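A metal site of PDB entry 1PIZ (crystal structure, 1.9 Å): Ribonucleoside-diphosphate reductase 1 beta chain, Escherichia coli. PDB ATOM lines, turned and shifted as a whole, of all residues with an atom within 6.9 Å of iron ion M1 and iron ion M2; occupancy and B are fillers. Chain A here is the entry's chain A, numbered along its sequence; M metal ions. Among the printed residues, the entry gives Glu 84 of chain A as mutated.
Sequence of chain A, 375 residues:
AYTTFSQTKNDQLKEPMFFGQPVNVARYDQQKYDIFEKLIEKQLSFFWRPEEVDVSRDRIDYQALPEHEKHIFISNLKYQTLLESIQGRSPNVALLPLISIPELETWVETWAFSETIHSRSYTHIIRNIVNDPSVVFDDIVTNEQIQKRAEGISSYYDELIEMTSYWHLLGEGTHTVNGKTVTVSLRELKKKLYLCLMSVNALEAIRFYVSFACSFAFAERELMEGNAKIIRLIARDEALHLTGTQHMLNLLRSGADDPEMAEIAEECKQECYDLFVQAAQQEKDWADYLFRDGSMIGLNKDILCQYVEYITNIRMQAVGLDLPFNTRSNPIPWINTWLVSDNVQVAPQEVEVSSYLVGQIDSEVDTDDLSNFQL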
ATOM      1  N   GLN A  80     -11.662  37.106   5.837  1.00  0.00           N
ATOM      2  CA  GLN A  80     -12.010  35.744   6.240  1.00  0.00           C
ATOM      3  C   GLN A  80     -13.434  35.735   6.797  1.00  0.00           C
ATOM      4  O   GLN A  80     -14.246  34.860   6.462  1.00  0.00           O
ATOM      5  CB  GLN A  80     -11.021  35.239   7.306  1.00  0.00           C
ATOM      6  CG  GLN A  80      -9.556  35.168   6.863  1.00  0.00           C
ATOM      7  CD  GLN A  80      -8.596  34.776   7.996  1.00  0.00           C
ATOM      8  OE1 GLN A  80      -8.661  35.325   9.099  1.00  0.00           O
ATOM      9  NE2 GLN A  80      -7.687  33.843   7.702  1.00  0.00           N
ATOM     10  N   LEU A  83     -15.963  35.892   3.994  1.00  0.00           N
ATOM     11  CA  LEU A  83     -16.109  34.596   3.325  1.00  0.00           C
ATOM     12  C   LEU A  83     -16.872  33.563   4.144  1.00  0.00           C
ATOM     13  O   LEU A  83     -17.649  32.793   3.591  1.00  0.00           O
ATOM     14  CB  LEU A  83     -14.727  34.035   2.953  1.00  0.00           C
ATOM     15  CG  LEU A  83     -13.924  34.789   1.891  1.00  0.00           C
ATOM     16  CD1 LEU A  83     -12.671  33.973   1.558  1.00  0.00           C
ATOM     17  CD2 LEU A  83     -14.768  34.995   0.636  1.00  0.00           C
ATOM     18  N   GLU A  84     -16.647  33.533   5.453  1.00  0.00           N
ATOM     19  CA  GLU A  84     -17.352  32.566   6.296  1.00  0.00           C
ATOM     20  C   GLU A  84     -18.828  32.949   6.406  1.00  0.00           C
ATOM     21  O   GLU A  84     -19.693  32.076   6.448  1.00  0.00           O
ATOM     22  CB  GLU A  84     -16.720  32.514   7.687  1.00  0.00           C
ATOM     23  CG  GLU A  84     -15.260  32.101   7.662  1.00  0.00           C
ATOM     24  CD  GLU A  84     -15.050  30.630   7.311  1.00  0.00           C
ATOM     25  OE1 GLU A  84     -16.002  29.980   6.856  1.00  0.00           O
ATOM     26  OE2 GLU A  84     -13.923  30.149   7.483  1.00  0.00           O
ATOM     27  N   GLN A  87     -20.236  31.686   3.220  1.00  0.00           N
ATOM     28  CA  GLN A  87     -20.205  30.222   3.166  1.00  0.00           C
ATOM     29  C   GLN A  87     -21.075  29.535   4.214  1.00  0.00           C
ATOM     30  O   GLN A  87     -21.369  28.346   4.097  1.00  0.00           O
ATOM     31  CB  GLN A  87     -18.759  29.721   3.272  1.00  0.00           C
ATOM     32  CG  GLN A  87     -17.928  29.905   1.991  1.00  0.00           C
ATOM     33  CD  GLN A  87     -18.642  29.413   0.748  1.00  0.00           C
ATOM     34  OE1 GLN A  87     -19.479  30.119   0.174  1.00  0.00           O
ATOM     35  NE2 GLN A  87     -18.346  28.190   0.332  1.00  0.00           N
ATOM     36  N   TRP A 111     -21.353  20.824   5.959  1.00  0.00           N
ATOM     37  CA  TRP A 111     -20.321  21.740   5.466  1.00  0.00           C
ATOM     38  C   TRP A 111     -20.704  23.177   5.845  1.00  0.00           C
ATOM     39  O   TRP A 111     -19.908  23.912   6.440  1.00  0.00           O
ATOM     40  CB  TRP A 111     -20.200  21.530   3.945  1.00  0.00           C
ATOM     41  CG  TRP A 111     -19.526  22.597   3.134  1.00  0.00           C
ATOM     42  CD1 TRP A 111     -18.666  23.565   3.567  1.00  0.00           C
ATOM     43  CD2 TRP A 111     -19.633  22.745   1.715  1.00  0.00           C
ATOM     44  NE1 TRP A 111     -18.230  24.320   2.491  1.00  0.00           N
ATOM     45  CE2 TRP A 111     -18.806  23.835   1.344  1.00  0.00           C
ATOM     46  CE3 TRP A 111     -20.358  22.071   0.717  1.00  0.00           C
ATOM     47  CZ2 TRP A 111     -18.681  24.257   0.012  1.00  0.00           C
ATOM     48  CZ3 TRP A 111     -20.225  22.488  -0.610  1.00  0.00           C
ATOM     49  CH2 TRP A 111     -19.391  23.577  -0.947  1.00  0.00           C
ATOM     50  N   SER A 114     -20.417  23.855   9.609  1.00  0.00           N
ATOM     51  CA  SER A 114     -19.042  24.046  10.062  1.00  0.00           C
ATOM     52  C   SER A 114     -18.569  25.458   9.735  1.00  0.00           C
ATOM     53  O   SER A 114     -17.749  26.021  10.457  1.00  0.00           O
ATOM     54  CB  SER A 114     -18.109  23.005   9.430  1.00  0.00           C
ATOM     55  OG  SER A 114     -17.898  23.266   8.060  1.00  0.00           O
ATOM     56  N   GLU A 115     -19.077  26.039   8.648  1.00  0.00           N
ATOM     57  CA  GLU A 115     -18.680  27.387   8.283  1.00  0.00           C
ATOM     58  C   GLU A 115     -19.237  28.375   9.319  1.00  0.00           C
ATOM     59  O   GLU A 115     -18.577  29.382   9.635  1.00  0.00           O
ATOM     60  CB  GLU A 115     -19.185  27.743   6.873  1.00  0.00           C
ATOM     61  CG  GLU A 115     -18.743  26.754   5.777  1.00  0.00           C
ATOM     62  CD  GLU A 115     -17.267  26.831   5.423  1.00  0.00           C
ATOM     63  OE1 GLU A 115     -16.428  27.039   6.340  1.00  0.00           O
ATOM     64  OE2 GLU A 115     -16.925  26.659   4.241  1.00  0.00           O
ATOM     65  N   THR A 116     -20.423  28.111   9.857  1.00  0.00           N
ATOM     66  CA  THR A 116     -20.988  29.014  10.876  1.00  0.00           C
ATOM     67  C   THR A 116     -20.159  28.937  12.149  1.00  0.00           C
ATOM     68  O   THR A 116     -20.062  29.915  12.898  1.00  0.00           O
ATOM     69  CB  THR A 116     -22.474  28.691  11.209  1.00  0.00           C
ATOM     70  OG1 THR A 116     -22.578  27.395  11.829  1.00  0.00           O
ATOM     71  CG2 THR A 116     -23.317  28.745   9.957  1.00  0.00           C
ATOM     72  N   HIS A 118     -16.986  28.578  12.081  1.00  0.00           N
ATOM     73  CA  HIS A 118     -15.835  29.417  11.756  1.00  0.00           C
ATOM     74  C   HIS A 118     -16.195  30.879  11.984  1.00  0.00           C
ATOM     75  O   HIS A 118     -15.391  31.653  12.519  1.00  0.00           O
ATOM     76  CB  HIS A 118     -15.411  29.183  10.308  1.00  0.00           C
ATOM     77  CG  HIS A 118     -14.968  27.775  10.023  1.00  0.00           C
ATOM     78  ND1 HIS A 118     -14.680  27.338   8.759  1.00  0.00           N
ATOM     79  CD2 HIS A 118     -14.785  26.717  10.848  1.00  0.00           C
ATOM     80  CE1 HIS A 118     -14.338  26.062   8.809  1.00  0.00           C
ATOM     81  NE2 HIS A 118     -14.396  25.660  10.068  1.00  0.00           N
ATOM     82  N   SER A 119     -17.392  31.273  11.571  1.00  0.00           N
ATOM     83  CA  SER A 119     -17.835  32.659  11.762  1.00  0.00           C
ATOM     84  C   SER A 119     -17.851  32.982  13.257  1.00  0.00           C
ATOM     85  O   SER A 119     -17.465  34.069  13.678  1.00  0.00           O
ATOM     86  CB  SER A 119     -19.258  32.856  11.203  1.00  0.00           C
ATOM     87  OG  SER A 119     -19.271  32.720   9.794  1.00  0.00           O
ATOM     88  N   TYR A 122     -14.446  33.731  14.608  1.00  0.00           N
ATOM     89  CA  TYR A 122     -13.943  35.068  14.303  1.00  0.00           C
ATOM     90  C   TYR A 122     -14.534  36.130  15.230  1.00  0.00           C
ATOM     91  O   TYR A 122     -13.867  37.108  15.568  1.00  0.00           O
ATOM     92  CB  TYR A 122     -14.203  35.398  12.831  1.00  0.00           C
ATOM     93  CG  TYR A 122     -13.232  34.683  11.915  1.00  0.00           C
ATOM     94  CD1 TYR A 122     -11.860  34.890  12.063  1.00  0.00           C
ATOM     95  CD2 TYR A 122     -13.669  33.801  10.937  1.00  0.00           C
ATOM     96  CE1 TYR A 122     -10.942  34.236  11.242  1.00  0.00           C
ATOM     97  CE2 TYR A 122     -12.747  33.127  10.110  1.00  0.00           C
ATOM     98  CZ  TYR A 122     -11.382  33.359  10.277  1.00  0.00           C
ATOM     99  OH  TYR A 122     -10.466  32.718   9.474  1.00  0.00           O
ATOM    100  N   GLU A 204     -12.982  27.920  -1.634  1.00  0.00           N
ATOM    101  CA  GLU A 204     -12.555  27.004  -0.573  1.00  0.00           C
ATOM    102  C   GLU A 204     -11.060  26.631  -0.634  1.00  0.00           C
ATOM    103  O   GLU A 204     -10.388  26.570   0.394  1.00  0.00           O
ATOM    104  CB  GLU A 204     -13.358  25.701  -0.642  1.00  0.00           C
ATOM    105  CG  GLU A 204     -14.882  25.803  -0.434  1.00  0.00           C
ATOM    106  CD  GLU A 204     -15.294  26.020   1.017  1.00  0.00           C
ATOM    107  OE1 GLU A 204     -14.512  25.671   1.928  1.00  0.00           O
ATOM    108  OE2 GLU A 204     -16.402  26.542   1.261  1.00  0.00           O
ATOM    109  N   PHE A 208      -9.321  30.975   0.797  1.00  0.00           N
ATOM    110  CA  PHE A 208      -9.114  30.706   2.223  1.00  0.00           C
ATOM    111  C   PHE A 208      -7.642  30.467   2.553  1.00  0.00           C
ATOM    112  O   PHE A 208      -7.151  30.930   3.588  1.00  0.00           O
ATOM    113  CB  PHE A 208      -9.930  29.496   2.690  1.00  0.00           C
ATOM    114  CG  PHE A 208     -11.362  29.809   3.060  1.00  0.00           C
ATOM    115  CD1 PHE A 208     -11.659  30.883   3.886  1.00  0.00           C
ATOM    116  CD2 PHE A 208     -12.402  28.994   2.608  1.00  0.00           C
ATOM    117  CE1 PHE A 208     -12.986  31.144   4.270  1.00  0.00           C
ATOM    118  CE2 PHE A 208     -13.717  29.245   2.983  1.00  0.00           C
ATOM    119  CZ  PHE A 208     -14.012  30.327   3.815  1.00  0.00           C
ATOM    120  N   PHE A 212      -4.833  32.141   5.118  1.00  0.00           N
ATOM    121  CA  PHE A 212      -4.192  31.384   6.186  1.00  0.00           C
ATOM    122  C   PHE A 212      -2.709  31.756   6.267  1.00  0.00           C
ATOM    123  O   PHE A 212      -2.160  31.878   7.353  1.00  0.00           O
ATOM    124  CB  PHE A 212      -4.299  29.868   5.958  1.00  0.00           C
ATOM    125  CG  PHE A 212      -5.700  29.342   5.993  1.00  0.00           C
ATOM    126  CD1 PHE A 212      -6.700  30.022   6.683  1.00  0.00           C
ATOM    127  CD2 PHE A 212      -6.022  28.149   5.356  1.00  0.00           C
ATOM    128  CE1 PHE A 212      -7.994  29.522   6.726  1.00  0.00           C
ATOM    129  CE2 PHE A 212      -7.312  27.644   5.386  1.00  0.00           C
ATOM    130  CZ  PHE A 212      -8.303  28.336   6.075  1.00  0.00           C
ATOM    131  N   ILE A 234      -9.691  25.698  11.598  1.00  0.00           N
ATOM    132  CA  ILE A 234     -10.476  26.087  10.435  1.00  0.00           C
ATOM    133  C   ILE A 234      -9.907  25.446   9.185  1.00  0.00           C
ATOM    134  O   ILE A 234     -10.637  24.865   8.380  1.00  0.00           O
ATOM    135  CB  ILE A 234     -10.487  27.620  10.257  1.00  0.00           C
ATOM    136  CG1 ILE A 234     -11.319  28.264  11.360  1.00  0.00           C
ATOM    137  CG2 ILE A 234     -11.048  27.988   8.888  1.00  0.00           C
ATOM    138  CD1 ILE A 234     -11.432  29.783  11.227  1.00  0.00           C
ATOM    139  N   ASP A 237     -10.840  21.956   8.567  1.00  0.00           N
ATOM    140  CA  ASP A 237     -12.196  21.818   8.029  1.00  0.00           C
ATOM    141  C   ASP A 237     -12.216  22.168   6.537  1.00  0.00           C
ATOM    142  O   ASP A 237     -12.843  21.474   5.743  1.00  0.00           O
ATOM    143  CB  ASP A 237     -13.186  22.724   8.787  1.00  0.00           C
ATOM    144  CG  ASP A 237     -13.399  22.303  10.225  1.00  0.00           C
ATOM    145  OD1 ASP A 237     -13.201  21.104  10.548  1.00  0.00           O
ATOM    146  OD2 ASP A 237     -13.792  23.172  11.042  1.00  0.00           O
ATOM    147  N   GLU A 238     -11.536  23.254   6.161  1.00  0.00           N
ATOM    148  CA  GLU A 238     -11.512  23.673   4.767  1.00  0.00           C
ATOM    149  C   GLU A 238     -10.936  22.572   3.866  1.00  0.00           C
ATOM    150  O   GLU A 238     -11.334  22.449   2.701  1.00  0.00           O
ATOM    151  CB  GLU A 238     -10.706  24.965   4.582  1.00  0.00           C
ATOM    152  CG  GLU A 238     -11.184  26.183   5.383  1.00  0.00           C
ATOM    153  CD  GLU A 238     -12.674  26.488   5.235  1.00  0.00           C
ATOM    154  OE1 GLU A 238     -13.308  25.983   4.282  1.00  0.00           O
ATOM    155  OE2 GLU A 238     -13.210  27.245   6.074  1.00  0.00           O
ATOM    156  N   ALA A 239     -10.008  21.792   4.402  1.00  0.00           N
ATOM    157  CA  ALA A 239      -9.410  20.709   3.627  1.00  0.00           C
ATOM    158  C   ALA A 239     -10.481  19.684   3.235  1.00  0.00           C
ATOM    159  O   ALA A 239     -10.467  19.138   2.131  1.00  0.00           O
ATOM    160  CB  ALA A 239      -8.296  20.029   4.428  1.00  0.00           C
ATOM    161  N   HIS A 241     -13.742  20.412   3.011  1.00  0.00           N
ATOM    162  CA  HIS A 241     -14.634  21.143   2.119  1.00  0.00           C
ATOM    163  C   HIS A 241     -14.133  21.128   0.683  1.00  0.00           C
ATOM    164  O   HIS A 241     -14.885  20.826  -0.242  1.00  0.00           O
ATOM    165  CB  HIS A 241     -14.805  22.584   2.602  1.00  0.00           C
ATOM    166  CG  HIS A 241     -15.345  22.703   3.994  1.00  0.00           C
ATOM    167  ND1 HIS A 241     -15.470  23.916   4.641  1.00  0.00           N
ATOM    168  CD2 HIS A 241     -15.791  21.766   4.868  1.00  0.00           C
ATOM    169  CE1 HIS A 241     -15.953  23.717   5.855  1.00  0.00           C
ATOM    170  NE2 HIS A 241     -16.160  22.419   6.018  1.00  0.00           N
ATOM    171  N   LEU A 242     -12.858  21.469   0.482  1.00  0.00           N
ATOM    172  CA  LEU A 242     -12.340  21.477  -0.885  1.00  0.00           C
ATOM    173  C   LEU A 242     -12.251  20.047  -1.422  1.00  0.00           C
ATOM    174  O   LEU A 242     -12.364  19.835  -2.630  1.00  0.00           O
ATOM    175  CB  LEU A 242     -10.988  22.192  -0.935  1.00  0.00           C
ATOM    176  CG  LEU A 242      -9.716  21.574  -0.360  1.00  0.00           C
ATOM    177  CD1 LEU A 242      -9.129  20.562  -1.339  1.00  0.00           C
ATOM    178  CD2 LEU A 242      -8.699  22.692  -0.115  1.00  0.00           C
HETATM  179 FE    FE M   1     -15.170  25.785   3.804  1.00  0.00          FE
HETATM  180 FE    FE M   2     -14.748  28.145   6.868  1.00  0.00          FE
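Iron ion M1 is bound by OE1 of Glu 238.
Iron ion M1 is bound by OE1 of Glu 204, at 2.0 Å.
Iron ion M1 is bound by OE2 of Glu 115, 2.0 Å away.
ND1 of His 241 is bound to iron ion M1.
The indole nitrogen of Trp 111 sits at hydrogen-bond distance from the side-chain carboxylate of Glu 204 (3.1 Å).
OG of Ser 119 sits close to O of Glu 84.
The backbone carbonyl oxygen (O) of Ser 114 lies close to a ring nitrogen (NE2) of His 118, 3.4 Å away.
NE2 of Gln 87 is in hydrogen-bond range of OE2 of Glu 204 (2.7 Å).
O of Trp 111 is in hydrogen-bond range of OG of Ser 114 (2.7 Å).
The backbone carbonyl oxygen (O) of Glu 115 is in hydrogen-bond range of the side-chain hydroxyl (OG) of Ser 119.
The indole nitrogen of Trp 111 sits close to the side-chain carboxylate of Glu 115 (3.2 Å).
A ring nitrogen (NE2) of His 241 sits close to the backbone carbonyl oxygen (O) of Asp 237 (3.5 Å).
OE2 of Glu 238 binds iron ion M2.
Iron ion M2 is bound by ND1 of His 118, 2.1 Å away.
Iron ion M2 is bound by OE1 of Glu 115 (2.1 Å).
OE1 of Glu 84 binds iron ion M2 (2.2 Å).
OE2 of Glu 84 binds iron ion M2 (2.3 Å).
Iron ion M2 has five donor atoms within binding distance.
Residues that only touch iron ion M1: Trp 111 (3.6 Å) and Phe 208 (3.8 Å).
Of the 20 residues printed, 6 come within 4 Å of iron ion M1.
Phe 208 touches iron ion M2.
Five residues have an atom within 4 Å of iron ion M2: Glu 84, Glu 115, His 118, Phe 208 and Glu 238.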
